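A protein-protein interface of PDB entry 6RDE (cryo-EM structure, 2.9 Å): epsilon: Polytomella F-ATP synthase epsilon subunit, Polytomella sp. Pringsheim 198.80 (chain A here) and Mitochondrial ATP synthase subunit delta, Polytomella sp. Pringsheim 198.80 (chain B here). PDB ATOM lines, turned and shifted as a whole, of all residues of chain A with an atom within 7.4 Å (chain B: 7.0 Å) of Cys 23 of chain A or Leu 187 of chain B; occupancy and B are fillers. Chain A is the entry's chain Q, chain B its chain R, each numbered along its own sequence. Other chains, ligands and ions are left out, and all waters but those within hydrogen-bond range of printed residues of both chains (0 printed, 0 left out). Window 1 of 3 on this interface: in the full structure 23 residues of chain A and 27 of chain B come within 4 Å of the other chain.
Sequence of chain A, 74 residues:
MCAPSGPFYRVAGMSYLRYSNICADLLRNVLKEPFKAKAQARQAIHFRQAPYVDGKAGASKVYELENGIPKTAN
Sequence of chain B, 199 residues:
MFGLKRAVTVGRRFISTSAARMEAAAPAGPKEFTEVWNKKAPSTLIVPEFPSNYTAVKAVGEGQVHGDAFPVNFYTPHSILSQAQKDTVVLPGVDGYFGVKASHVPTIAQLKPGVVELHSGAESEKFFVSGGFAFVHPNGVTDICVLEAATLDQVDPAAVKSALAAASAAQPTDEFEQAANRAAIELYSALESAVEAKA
The side-chain hydroxyl of Ser 20 of chain A sits at hydrogen-bond distance from the backbone carbonyl oxygen of Gly 131 of chain B.
OE2 of Glu 148 of chain B lies within salt-bridge range of NE of Arg 28 of chain A, at 2.4 Å.
The side-chain hydroxyl (OH) of Tyr 19 of chain A sits at hydrogen-bond distance from the side-chain carboxylate (OE2) of Glu 186 of chain B (3.4 Å).
The backbone carbonyl oxygen (O) of Gly 114 of chain B is in hydrogen-bond range of the backbone NH (N) of Val 129 of chain B, 2.7 Å away.
The backbone carbonyl oxygen (O) of Tyr 19 of chain A lies within hydrogen-bond range of the side-chain sulfur (SG) of Cys 23 of chain A (3.3 Å).
O of Glu 148 of chain B sits at hydrogen-bond distance from N of Ser 130 of chain B (2.8 Å).
ND2 of Asn 21 of chain A is in hydrogen-bond range of O of Leu 17 of chain A.
The side-chain carboxylate (OD1) of Asp 25 of chain A is in salt-bridge range of the guanidinium group (NH1) of Arg 28 of chain A.
N of Ala 183 of chain B touches CE1 of Phe 8 of chain A, 3.7 Å away.
Ala 183 of chain B touches Tyr 19 of chain A.
O of Cys 23 of chain A touches CB of Ser 130 of chain B (3.3 Å).
Leu 147 of chain B touches Ala 24 of chain A.
Ala 184 of chain B touches Leu 26 of chain A (CA to CD1, 3.8 Å).
Leu 27 of chain A touches Phe 128 of chain B.
Leu 27 of chain A touches Val 129 of chain B (CD2 to C, 3.9 Å).
N of Leu 27 of chain A touches CD2 of Leu 187 of chain B, at 3.97 Å.
Leu 191 of chain B touches Leu 27 of chain A.
Tyr 188 of chain B touches Val 30 of chain A.
Of the printed residues of chain B, Cys 23 of chain A touches Ser 130 and Leu 187.
Of chain A, only Cys 23, Leu 26 and Leu 27 come within 4 Å of Leu 187 of chain B.
Of the printed residues of chain B, Tyr 19 of chain A touches Ala 183 (3.6 Å) and Glu 186 (3.4 Å).
Of the printed residues of chain B, Phe 8 of chain A touches Arg 182 (3.4 Å), Ala 183 (3.7 Å) and Glu 186 (3.3 Å).
Printed residues of chain A within 4 Å of Ala 183 of chain B: Phe 8 (3.7 Å) and Tyr 19 (3.6 Å).
Printed residues of chain A within 4 Å of Tyr 188 of chain B: Leu 26 (3.3 Å) and Val 30 (3.7 Å).
Of the printed residues of chain B, Ala 24 of chain A touches Ser 130, Leu 147 and Glu 148.
Ser 189 of chain B touches none of the printed residues of chain A.
The nearest residue of chain A that does not touch Leu 187 of chain B is Ile 22 of chain A (4.8 Å).
Of the 16 printed residues of chain A, 10 touch a printed residue of chain B.
Of the 20 printed residues of chain B, 13 touch a printed residue of chain A.
Printed residues of chain B that touch a printed residue of chain A: Phe 128, Val 129, Ser 130, Gly 131, Leu 147, Glu 148, Arg 182, Ala 183, Ala 184, Glu 186, Leu 187, Tyr 188 and Leu 191.
Among the printed residues, Asp or Glu carboxylates within 4 Å of a Lys or Arg side-chain nitrogen of the other chain: Arg 28 of chain A with Glu 148 of chain B.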
ATOM      1  N   PHE A   8       6.262 -25.722   7.948  1.00  0.00           N
ATOM      2  CA  PHE A   8       6.239 -25.707   6.492  1.00  0.00           C
ATOM      3  C   PHE A   8       6.475 -24.324   5.910  1.00  0.00           C
ATOM      4  O   PHE A   8       6.908 -24.219   4.760  1.00  0.00           O
ATOM      5  CB  PHE A   8       4.920 -26.265   5.971  1.00  0.00           C
ATOM      6  CG  PHE A   8       3.742 -25.354   6.161  1.00  0.00           C
ATOM      7  CD1 PHE A   8       3.244 -24.612   5.102  1.00  0.00           C
ATOM      8  CD2 PHE A   8       3.104 -25.278   7.381  1.00  0.00           C
ATOM      9  CE1 PHE A   8       2.162 -23.791   5.273  1.00  0.00           C
ATOM     10  CE2 PHE A   8       2.018 -24.458   7.551  1.00  0.00           C
ATOM     11  CZ  PHE A   8       1.547 -23.715   6.497  1.00  0.00           C
ATOM     12  N   LEU A  17       5.936 -13.912  10.440  1.00  0.00           N
ATOM     13  CA  LEU A  17       5.164 -12.713  10.157  1.00  0.00           C
ATOM     14  C   LEU A  17       4.677 -12.690   8.726  1.00  0.00           C
ATOM     15  O   LEU A  17       3.604 -12.152   8.449  1.00  0.00           O
ATOM     16  CB  LEU A  17       6.003 -11.480  10.428  1.00  0.00           C
ATOM     17  CG  LEU A  17       6.385 -11.271  11.875  1.00  0.00           C
ATOM     18  CD1 LEU A  17       7.722 -10.589  11.882  1.00  0.00           C
ATOM     19  CD2 LEU A  17       5.326 -10.432  12.532  1.00  0.00           C
ATOM     20  N   ARG A  18       5.440 -13.263   7.807  1.00  0.00           N
ATOM     21  CA  ARG A  18       4.943 -13.352   6.448  1.00  0.00           C
ATOM     22  C   ARG A  18       3.897 -14.438   6.308  1.00  0.00           C
ATOM     23  O   ARG A  18       2.977 -14.298   5.500  1.00  0.00           O
ATOM     24  CB  ARG A  18       6.083 -13.597   5.476  1.00  0.00           C
ATOM     25  CG  ARG A  18       5.777 -13.051   4.123  1.00  0.00           C
ATOM     26  CD  ARG A  18       6.980 -13.129   3.246  1.00  0.00           C
ATOM     27  NE  ARG A  18       7.955 -12.088   3.526  1.00  0.00           N
ATOM     28  CZ  ARG A  18       8.365 -11.215   2.621  1.00  0.00           C
ATOM     29  NH1 ARG A  18       7.875 -11.267   1.391  1.00  0.00           N
ATOM     30  NH2 ARG A  18       9.265 -10.300   2.941  1.00  0.00           N
ATOM     31  N   TYR A  19       4.008 -15.509   7.086  1.00  0.00           N
ATOM     32  CA  TYR A  19       3.015 -16.569   7.019  1.00  0.00           C
ATOM     33  C   TYR A  19       1.711 -16.135   7.662  1.00  0.00           C
ATOM     34  O   TYR A  19       0.631 -16.360   7.110  1.00  0.00           O
ATOM     35  CB  TYR A  19       3.548 -17.832   7.698  1.00  0.00           C
ATOM     36  CG  TYR A  19       2.469 -18.779   8.173  1.00  0.00           C
ATOM     37  CD1 TYR A  19       2.147 -18.878   9.525  1.00  0.00           C
ATOM     38  CD2 TYR A  19       1.782 -19.579   7.273  1.00  0.00           C
ATOM     39  CE1 TYR A  19       1.167 -19.726   9.957  1.00  0.00           C
ATOM     40  CE2 TYR A  19       0.804 -20.441   7.702  1.00  0.00           C
ATOM     41  CZ  TYR A  19       0.500 -20.511   9.045  1.00  0.00           C
ATOM     42  OH  TYR A  19      -0.481 -21.374   9.476  1.00  0.00           O
ATOM     43  N   SER A  20       1.793 -15.526   8.837  1.00  0.00           N
ATOM     44  CA  SER A  20       0.591 -15.250   9.600  1.00  0.00           C
ATOM     45  C   SER A  20      -0.137 -14.016   9.101  1.00  0.00           C
ATOM     46  O   SER A  20      -1.318 -13.848   9.408  1.00  0.00           O
ATOM     47  CB  SER A  20       0.940 -15.098  11.075  1.00  0.00           C
ATOM     48  OG  SER A  20      -0.229 -15.019  11.857  1.00  0.00           O
ATOM     49  N   ASN A  21       0.536 -13.154   8.339  1.00  0.00           N
ATOM     50  CA  ASN A  21      -0.162 -12.076   7.655  1.00  0.00           C
ATOM     51  C   ASN A  21      -0.874 -12.567   6.407  1.00  0.00           C
ATOM     52  O   ASN A  21      -1.914 -12.012   6.042  1.00  0.00           O
ATOM     53  CB  ASN A  21       0.808 -10.966   7.274  1.00  0.00           C
ATOM     54  CG  ASN A  21       1.122 -10.059   8.425  1.00  0.00           C
ATOM     55  OD1 ASN A  21       0.274  -9.295   8.876  1.00  0.00           O
ATOM     56  ND2 ASN A  21       2.342 -10.140   8.918  1.00  0.00           N
ATOM     57  N   ILE A  22      -0.316 -13.580   5.742  1.00  0.00           N
ATOM     58  CA  ILE A  22      -0.980 -14.207   4.604  1.00  0.00           C
ATOM     59  C   ILE A  22      -2.301 -14.831   5.039  1.00  0.00           C
ATOM     60  O   ILE A  22      -3.335 -14.652   4.385  1.00  0.00           O
ATOM     61  CB  ILE A  22      -0.035 -15.234   3.952  1.00  0.00           C
ATOM     62  CG1 ILE A  22       0.902 -14.541   2.974  1.00  0.00           C
ATOM     63  CG2 ILE A  22      -0.792 -16.320   3.223  1.00  0.00           C
ATOM     64  CD1 ILE A  22       2.021 -15.424   2.490  1.00  0.00           C
ATOM     65  N   CYS A  23      -2.304 -15.516   6.183  1.00  0.00           N
ATOM     66  CA  CYS A  23      -3.551 -16.055   6.713  1.00  0.00           C
ATOM     67  C   CYS A  23      -4.471 -14.960   7.227  1.00  0.00           C
ATOM     68  O   CYS A  23      -5.670 -15.192   7.396  1.00  0.00           O
ATOM     69  CB  CYS A  23      -3.263 -17.069   7.816  1.00  0.00           C
ATOM     70  SG  CYS A  23      -2.033 -18.308   7.384  1.00  0.00           S
ATOM     71  N   ALA A  24      -3.934 -13.775   7.509  1.00  0.00           N
ATOM     72  CA  ALA A  24      -4.784 -12.627   7.776  1.00  0.00           C
ATOM     73  C   ALA A  24      -5.178 -11.915   6.494  1.00  0.00           C
ATOM     74  O   ALA A  24      -6.239 -11.287   6.446  1.00  0.00           O
ATOM     75  CB  ALA A  24      -4.082 -11.662   8.725  1.00  0.00           C
ATOM     76  N   ASP A  25      -4.337 -11.998   5.458  1.00  0.00           N
ATOM     77  CA  ASP A  25      -4.692 -11.463   4.145  1.00  0.00           C
ATOM     78  C   ASP A  25      -5.889 -12.197   3.563  1.00  0.00           C
ATOM     79  O   ASP A  25      -6.858 -11.574   3.118  1.00  0.00           O
ATOM     80  CB  ASP A  25      -3.503 -11.579   3.188  1.00  0.00           C
ATOM     81  CG  ASP A  25      -2.553 -10.404   3.281  1.00  0.00           C
ATOM     82  OD1 ASP A  25      -2.754  -9.529   4.149  1.00  0.00           O
ATOM     83  OD2 ASP A  25      -1.585 -10.368   2.495  1.00  0.00           O
ATOM     84  N   LEU A  26      -5.841 -13.528   3.566  1.00  0.00           N
ATOM     85  CA  LEU A  26      -6.889 -14.311   2.931  1.00  0.00           C
ATOM     86  C   LEU A  26      -8.163 -14.362   3.756  1.00  0.00           C
ATOM     87  O   LEU A  26      -9.225 -14.652   3.203  1.00  0.00           O
ATOM     88  CB  LEU A  26      -6.385 -15.725   2.659  1.00  0.00           C
ATOM     89  CG  LEU A  26      -5.094 -15.853   1.854  1.00  0.00           C
ATOM     90  CD1 LEU A  26      -4.454 -17.203   2.080  1.00  0.00           C
ATOM     91  CD2 LEU A  26      -5.357 -15.625   0.382  1.00  0.00           C
ATOM     92  N   LEU A  27      -8.093 -14.092   5.056  1.00  0.00           N
ATOM     93  CA  LEU A  27      -9.312 -14.056   5.852  1.00  0.00           C
ATOM     94  C   LEU A  27     -10.066 -12.745   5.671  1.00  0.00           C
ATOM     95  O   LEU A  27     -11.296 -12.723   5.787  1.00  0.00           O
ATOM     96  CB  LEU A  27      -8.989 -14.292   7.328  1.00  0.00           C
ATOM     97  CG  LEU A  27     -10.185 -14.448   8.274  1.00  0.00           C
ATOM     98  CD1 LEU A  27     -11.108 -15.511   7.739  1.00  0.00           C
ATOM     99  CD2 LEU A  27      -9.781 -14.769   9.692  1.00  0.00           C
ATOM    100  N   ARG A  28      -9.354 -11.653   5.371  1.00  0.00           N
ATOM    101  CA  ARG A  28     -10.016 -10.370   5.147  1.00  0.00           C
ATOM    102  C   ARG A  28     -10.851 -10.382   3.876  1.00  0.00           C
ATOM    103  O   ARG A  28     -11.871  -9.688   3.804  1.00  0.00           O
ATOM    104  CB  ARG A  28      -8.989  -9.241   5.073  1.00  0.00           C
ATOM    105  CG  ARG A  28      -8.405  -8.836   6.405  1.00  0.00           C
ATOM    106  CD  ARG A  28      -7.365  -7.738   6.269  1.00  0.00           C
ATOM    107  NE  ARG A  28      -6.356  -7.804   7.325  1.00  0.00           N
ATOM    108  CZ  ARG A  28      -5.053  -7.944   7.105  1.00  0.00           C
ATOM    109  NH1 ARG A  28      -4.595  -8.030   5.866  1.00  0.00           N
ATOM    110  NH2 ARG A  28      -4.201  -8.003   8.118  1.00  0.00           N
ATOM    111  N   VAL A  30     -12.761 -12.658   2.667  1.00  0.00           N
ATOM    112  CA  VAL A  30     -13.930 -13.528   2.654  1.00  0.00           C
ATOM    113  C   VAL A  30     -14.845 -13.051   3.782  1.00  0.00           C
ATOM    114  O   VAL A  30     -15.466 -13.840   4.501  1.00  0.00           O
ATOM    115  CB  VAL A  30     -13.517 -15.013   2.773  1.00  0.00           C
ATOM    116  CG1 VAL A  30     -14.632 -15.943   2.320  1.00  0.00           C
ATOM    117  CG2 VAL A  30     -12.268 -15.302   1.958  1.00  0.00           C
ATOM    118  N   ILE A  69       0.316  -8.314   2.179  1.00  0.00           N
ATOM    119  CA  ILE A  69       1.765  -8.546   2.174  1.00  0.00           C
ATOM    120  C   ILE A  69       2.153  -9.201   0.850  1.00  0.00           C
ATOM    121  O   ILE A  69       1.277  -9.766   0.170  1.00  0.00           O
ATOM    122  CB  ILE A  69       2.154  -9.410   3.389  1.00  0.00           C
ATOM    123  CG1 ILE A  69       3.482  -8.962   3.999  1.00  0.00           C
ATOM    124  CG2 ILE A  69       2.244 -10.893   3.045  1.00  0.00           C
ATOM    125  CD1 ILE A  69       3.686  -9.451   5.400  1.00  0.00           C
ATOM    126  N   LYS A  71       2.906 -12.017  -1.293  1.00  0.00           N
ATOM    127  CA  LYS A  71       2.898 -13.473  -1.306  1.00  0.00           C
ATOM    128  C   LYS A  71       4.099 -14.057  -2.037  1.00  0.00           C
ATOM    129  O   LYS A  71       4.412 -15.234  -1.835  1.00  0.00           O
ATOM    130  CB  LYS A  71       1.623 -14.003  -1.966  1.00  0.00           C
ATOM    131  CG  LYS A  71       0.324 -13.648  -1.279  1.00  0.00           C
ATOM    132  CD  LYS A  71      -0.804 -14.526  -1.807  1.00  0.00           C
ATOM    133  CE  LYS A  71      -2.115 -14.308  -1.057  1.00  0.00           C
ATOM    134  NZ  LYS A  71      -2.902 -13.153  -1.564  1.00  0.00           N
ATOM    135  N   PRO B 113      -5.633 -21.827  11.732  1.00  0.00           N
ATOM    136  CA  PRO B 113      -6.923 -21.192  11.432  1.00  0.00           C
ATOM    137  C   PRO B 113      -8.123 -21.976  11.937  1.00  0.00           C
ATOM    138  O   PRO B 113      -8.390 -23.084  11.472  1.00  0.00           O
ATOM    139  CB  PRO B 113      -6.918 -21.128   9.908  1.00  0.00           C
ATOM    140  CG  PRO B 113      -5.513 -20.956   9.567  1.00  0.00           C
ATOM    141  CD  PRO B 113      -4.704 -21.682  10.594  1.00  0.00           C
ATOM    142  N   GLY B 114      -8.833 -21.414  12.901  1.00  0.00           N
ATOM    143  CA  GLY B 114      -9.958 -22.097  13.493  1.00  0.00           C
ATOM    144  C   GLY B 114     -10.813 -21.126  14.267  1.00  0.00           C
ATOM    145  O   GLY B 114     -10.694 -19.912  14.106  1.00  0.00           O
ATOM    146  N   PHE B 128     -13.942 -16.755  14.370  1.00  0.00           N
ATOM    147  CA  PHE B 128     -13.017 -17.511  13.536  1.00  0.00           C
ATOM    148  C   PHE B 128     -11.750 -16.688  13.345  1.00  0.00           C
ATOM    149  O   PHE B 128     -11.799 -15.576  12.815  1.00  0.00           O
ATOM    150  CB  PHE B 128     -13.632 -17.855  12.183  1.00  0.00           C
ATOM    151  CG  PHE B 128     -12.719 -18.645  11.294  1.00  0.00           C
ATOM    152  CD1 PHE B 128     -12.560 -20.005  11.481  1.00  0.00           C
ATOM    153  CD2 PHE B 128     -12.027 -18.031  10.265  1.00  0.00           C
ATOM    154  CE1 PHE B 128     -11.719 -20.730  10.665  1.00  0.00           C
ATOM    155  CE2 PHE B 128     -11.190 -18.749   9.453  1.00  0.00           C
ATOM    156  CZ  PHE B 128     -11.033 -20.098   9.651  1.00  0.00           C
ATOM    157  N   VAL B 129     -10.617 -17.242  13.754  1.00  0.00           N
ATOM    158  CA  VAL B 129      -9.367 -16.508  13.780  1.00  0.00           C
ATOM    159  C   VAL B 129      -8.478 -16.973  12.639  1.00  0.00           C
ATOM    160  O   VAL B 129      -8.659 -18.048  12.066  1.00  0.00           O
ATOM    161  CB  VAL B 129      -8.660 -16.663  15.136  1.00  0.00           C
ATOM    162  CG1 VAL B 129      -9.635 -16.395  16.223  1.00  0.00           C
ATOM    163  CG2 VAL B 129      -8.095 -18.049  15.291  1.00  0.00           C
ATOM    164  N   SER B 130      -7.506 -16.139  12.307  1.00  0.00           N
ATOM    165  CA  SER B 130      -6.616 -16.397  11.191  1.00  0.00           C
ATOM    166  C   SER B 130      -5.442 -17.287  11.554  1.00  0.00           C
ATOM    167  O   SER B 130      -4.795 -17.827  10.653  1.00  0.00           O
ATOM    168  CB  SER B 130      -6.074 -15.081  10.642  1.00  0.00           C
ATOM    169  OG  SER B 130      -4.947 -14.664  11.396  1.00  0.00           O
ATOM    170  N   GLY B 131      -5.139 -17.441  12.835  1.00  0.00           N
ATOM    171  CA  GLY B 131      -3.955 -18.166  13.235  1.00  0.00           C
ATOM    172  C   GLY B 131      -2.990 -17.300  14.010  1.00  0.00           C
ATOM    173  O   GLY B 131      -2.508 -16.282  13.508  1.00  0.00           O
ATOM    174  N   LEU B 147      -4.040 -12.496  14.630  1.00  0.00           N
ATOM    175  CA  LEU B 147      -3.961 -11.313  13.784  1.00  0.00           C
ATOM    176  C   LEU B 147      -5.347 -10.863  13.345  1.00  0.00           C
ATOM    177  O   LEU B 147      -5.809  -9.787  13.731  1.00  0.00           O
ATOM    178  CB  LEU B 147      -3.072 -11.568  12.565  1.00  0.00           C
ATOM    179  CG  LEU B 147      -1.588 -11.237  12.698  1.00  0.00           C
ATOM    180  CD1 LEU B 147      -0.866 -12.258  13.519  1.00  0.00           C
ATOM    181  CD2 LEU B 147      -0.962 -11.153  11.345  1.00  0.00           C
ATOM    182  N   GLU B 148      -6.038 -11.695  12.580  1.00  0.00           N
ATOM    183  CA  GLU B 148      -7.349 -11.365  12.052  1.00  0.00           C
ATOM    184  C   GLU B 148      -8.378 -12.239  12.742  1.00  0.00           C
ATOM    185  O   GLU B 148      -8.205 -13.457  12.822  1.00  0.00           O
ATOM    186  CB  GLU B 148      -7.396 -11.568  10.543  1.00  0.00           C
ATOM    187  CG  GLU B 148      -8.434 -10.725   9.843  1.00  0.00           C
ATOM    188  CD  GLU B 148      -8.087  -9.249   9.847  1.00  0.00           C
ATOM    189  OE1 GLU B 148      -8.931  -8.435  10.277  1.00  0.00           O
ATOM    190  OE2 GLU B 148      -6.971  -8.897   9.407  1.00  0.00           O
ATOM    191  N   ASN B 181       0.330 -21.793  -0.701  1.00  0.00           N
ATOM    192  CA  ASN B 181      -0.880 -22.517  -1.069  1.00  0.00           C
ATOM    193  C   ASN B 181      -1.314 -23.477   0.024  1.00  0.00           C
ATOM    194  O   ASN B 181      -2.516 -23.619   0.260  1.00  0.00           O
ATOM    195  CB  ASN B 181      -0.684 -23.290  -2.371  1.00  0.00           C
ATOM    196  CG  ASN B 181      -1.975 -23.493  -3.119  1.00  0.00           C
ATOM    197  OD1 ASN B 181      -2.897 -22.684  -3.019  1.00  0.00           O
ATOM    198  ND2 ASN B 181      -2.051 -24.575  -3.883  1.00  0.00           N
ATOM    199  N   ARG B 182      -0.361 -24.129   0.698  1.00  0.00           N
ATOM    200  CA  ARG B 182      -0.709 -25.004   1.813  1.00  0.00           C
ATOM    201  C   ARG B 182      -1.331 -24.213   2.949  1.00  0.00           C
ATOM    202  O   ARG B 182      -2.313 -24.655   3.555  1.00  0.00           O
ATOM    203  CB  ARG B 182       0.522 -25.755   2.303  1.00  0.00           C
ATOM    204  CG  ARG B 182       0.210 -26.692   3.441  1.00  0.00           C
ATOM    205  CD  ARG B 182       1.395 -27.515   3.858  1.00  0.00           C
ATOM    206  NE  ARG B 182       1.306 -27.829   5.273  1.00  0.00           N
ATOM    207  CZ  ARG B 182       2.183 -28.574   5.923  1.00  0.00           C
ATOM    208  NH1 ARG B 182       3.218 -29.090   5.278  1.00  0.00           N
ATOM    209  NH2 ARG B 182       2.021 -28.801   7.217  1.00  0.00           N
ATOM    210  N   ALA B 183      -0.809 -23.013   3.204  1.00  0.00           N
ATOM    211  CA  ALA B 183      -1.460 -22.077   4.106  1.00  0.00           C
ATOM    212  C   ALA B 183      -2.777 -21.553   3.551  1.00  0.00           C
ATOM    213  O   ALA B 183      -3.633 -21.127   4.331  1.00  0.00           O
ATOM    214  CB  ALA B 183      -0.526 -20.906   4.396  1.00  0.00           C
ATOM    215  N   ALA B 184      -2.963 -21.578   2.229  1.00  0.00           N
ATOM    216  CA  ALA B 184      -4.178 -21.008   1.662  1.00  0.00           C
ATOM    217  C   ALA B 184      -5.386 -21.914   1.863  1.00  0.00           C
ATOM    218  O   ALA B 184      -6.431 -21.441   2.322  1.00  0.00           O
ATOM    219  CB  ALA B 184      -3.994 -20.699   0.177  1.00  0.00           C
ATOM    220  N   ILE B 185      -5.276 -23.208   1.545  1.00  0.00           N
ATOM    221  CA  ILE B 185      -6.476 -24.038   1.618  1.00  0.00           C
ATOM    222  C   ILE B 185      -6.823 -24.362   3.068  1.00  0.00           C
ATOM    223  O   ILE B 185      -8.004 -24.471   3.406  1.00  0.00           O
ATOM    224  CB  ILE B 185      -6.367 -25.333   0.787  1.00  0.00           C
ATOM    225  CG1 ILE B 185      -5.744 -25.100  -0.583  1.00  0.00           C
ATOM    226  CG2 ILE B 185      -7.745 -25.895   0.501  1.00  0.00           C
ATOM    227  CD1 ILE B 185      -4.502 -25.904  -0.829  1.00  0.00           C
ATOM    228  N   GLU B 186      -5.819 -24.466   3.949  1.00  0.00           N
ATOM    229  CA  GLU B 186      -6.072 -24.895   5.323  1.00  0.00           C
ATOM    230  C   GLU B 186      -6.820 -23.832   6.117  1.00  0.00           C
ATOM    231  O   GLU B 186      -7.510 -24.156   7.092  1.00  0.00           O
ATOM    232  CB  GLU B 186      -4.756 -25.254   6.018  1.00  0.00           C
ATOM    233  CG  GLU B 186      -3.854 -24.074   6.349  1.00  0.00           C
ATOM    234  CD  GLU B 186      -2.505 -24.498   6.890  1.00  0.00           C
ATOM    235  OE1 GLU B 186      -2.250 -25.715   6.952  1.00  0.00           O
ATOM    236  OE2 GLU B 186      -1.702 -23.616   7.253  1.00  0.00           O
ATOM    237  N   LEU B 187      -6.715 -22.569   5.703  1.00  0.00           N
ATOM    238  CA  LEU B 187      -7.524 -21.523   6.306  1.00  0.00           C
ATOM    239  C   LEU B 187      -8.933 -21.544   5.744  1.00  0.00           C
ATOM    240  O   LEU B 187      -9.905 -21.313   6.471  1.00  0.00           O
ATOM    241  CB  LEU B 187      -6.859 -20.171   6.083  1.00  0.00           C
ATOM    242  CG  LEU B 187      -7.667 -18.879   6.125  1.00  0.00           C
ATOM    243  CD1 LEU B 187      -8.174 -18.556   7.511  1.00  0.00           C
ATOM    244  CD2 LEU B 187      -6.770 -17.795   5.628  1.00  0.00           C
ATOM    245  N   TYR B 188      -9.061 -21.831   4.453  1.00  0.00           N
ATOM    246  CA  TYR B 188     -10.376 -21.900   3.836  1.00  0.00           C
ATOM    247  C   TYR B 188     -11.127 -23.156   4.256  1.00  0.00           C
ATOM    248  O   TYR B 188     -12.330 -23.091   4.519  1.00  0.00           O
ATOM    249  CB  TYR B 188     -10.240 -21.844   2.315  1.00  0.00           C
ATOM    250  CG  TYR B 188      -9.795 -20.497   1.801  1.00  0.00           C
ATOM    251  CD1 TYR B 188     -10.256 -19.324   2.384  1.00  0.00           C
ATOM    252  CD2 TYR B 188      -8.920 -20.399   0.733  1.00  0.00           C
ATOM    253  CE1 TYR B 188      -9.847 -18.092   1.917  1.00  0.00           C
ATOM    254  CE2 TYR B 188      -8.503 -19.178   0.265  1.00  0.00           C
ATOM    255  CZ  TYR B 188      -8.974 -18.027   0.856  1.00  0.00           C
ATOM    256  OH  TYR B 188      -8.562 -16.803   0.381  1.00  0.00           O
ATOM    257  N   SER B 189     -10.431 -24.299   4.331  1.00  0.00           N
ATOM    258  CA  SER B 189     -11.088 -25.571   4.619  1.00  0.00           C
ATOM    259  C   SER B 189     -11.639 -25.618   6.033  1.00  0.00           C
ATOM    260  O   SER B 189     -12.707 -26.194   6.261  1.00  0.00           O
ATOM    261  CB  SER B 189     -10.118 -26.726   4.416  1.00  0.00           C
ATOM    262  OG  SER B 189      -9.679 -26.776   3.075  1.00  0.00           O
ATOM    263  N   ALA B 190     -10.944 -25.004   6.983  1.00  0.00           N
ATOM    264  CA  ALA B 190     -11.475 -24.888   8.331  1.00  0.00           C
ATOM    265  C   ALA B 190     -12.524 -23.798   8.448  1.00  0.00           C
ATOM    266  O   ALA B 190     -13.122 -23.656   9.513  1.00  0.00           O
ATOM    267  CB  ALA B 190     -10.346 -24.628   9.322  1.00  0.00           C
ATOM    268  N   LEU B 191     -12.744 -23.022   7.389  1.00  0.00           N
ATOM    269  CA  LEU B 191     -13.814 -22.036   7.352  1.00  0.00           C
ATOM    270  C   LEU B 191     -15.099 -22.575   6.732  1.00  0.00           C
ATOM    271  O   LEU B 191     -16.181 -22.081   7.067  1.00  0.00           O
ATOM    272  CB  LEU B 191     -13.339 -20.790   6.597  1.00  0.00           C
ATOM    273  CG  LEU B 191     -14.124 -19.486   6.720  1.00  0.00           C
ATOM    274  CD1 LEU B 191     -14.665 -19.281   8.128  1.00  0.00           C
ATOM    275  CD2 LEU B 191     -13.249 -18.319   6.302  1.00  0.00           C
ATOM    276  N   GLU B 192     -15.010 -23.572   5.842  1.00  0.00           N
ATOM    277  CA  GLU B 192     -16.204 -24.303   5.420  1.00  0.00           C
ATOM    278  C   GLU B 192     -16.833 -25.015   6.602  1.00  0.00           C
ATOM    279  O   GLU B 192     -18.034 -24.891   6.851  1.00  0.00           O
ATOM    280  CB  GLU B 192     -15.869 -25.329   4.335  1.00  0.00           C
ATOM    281  CG  GLU B 192     -14.769 -24.941   3.394  1.00  0.00           C
ATOM    282  CD  GLU B 192     -15.104 -23.712   2.588  1.00  0.00           C
ATOM    283  OE1 GLU B 192     -16.278 -23.549   2.193  1.00  0.00           O
ATOM    284  OE2 GLU B 192     -14.184 -22.907   2.354  1.00  0.00           O
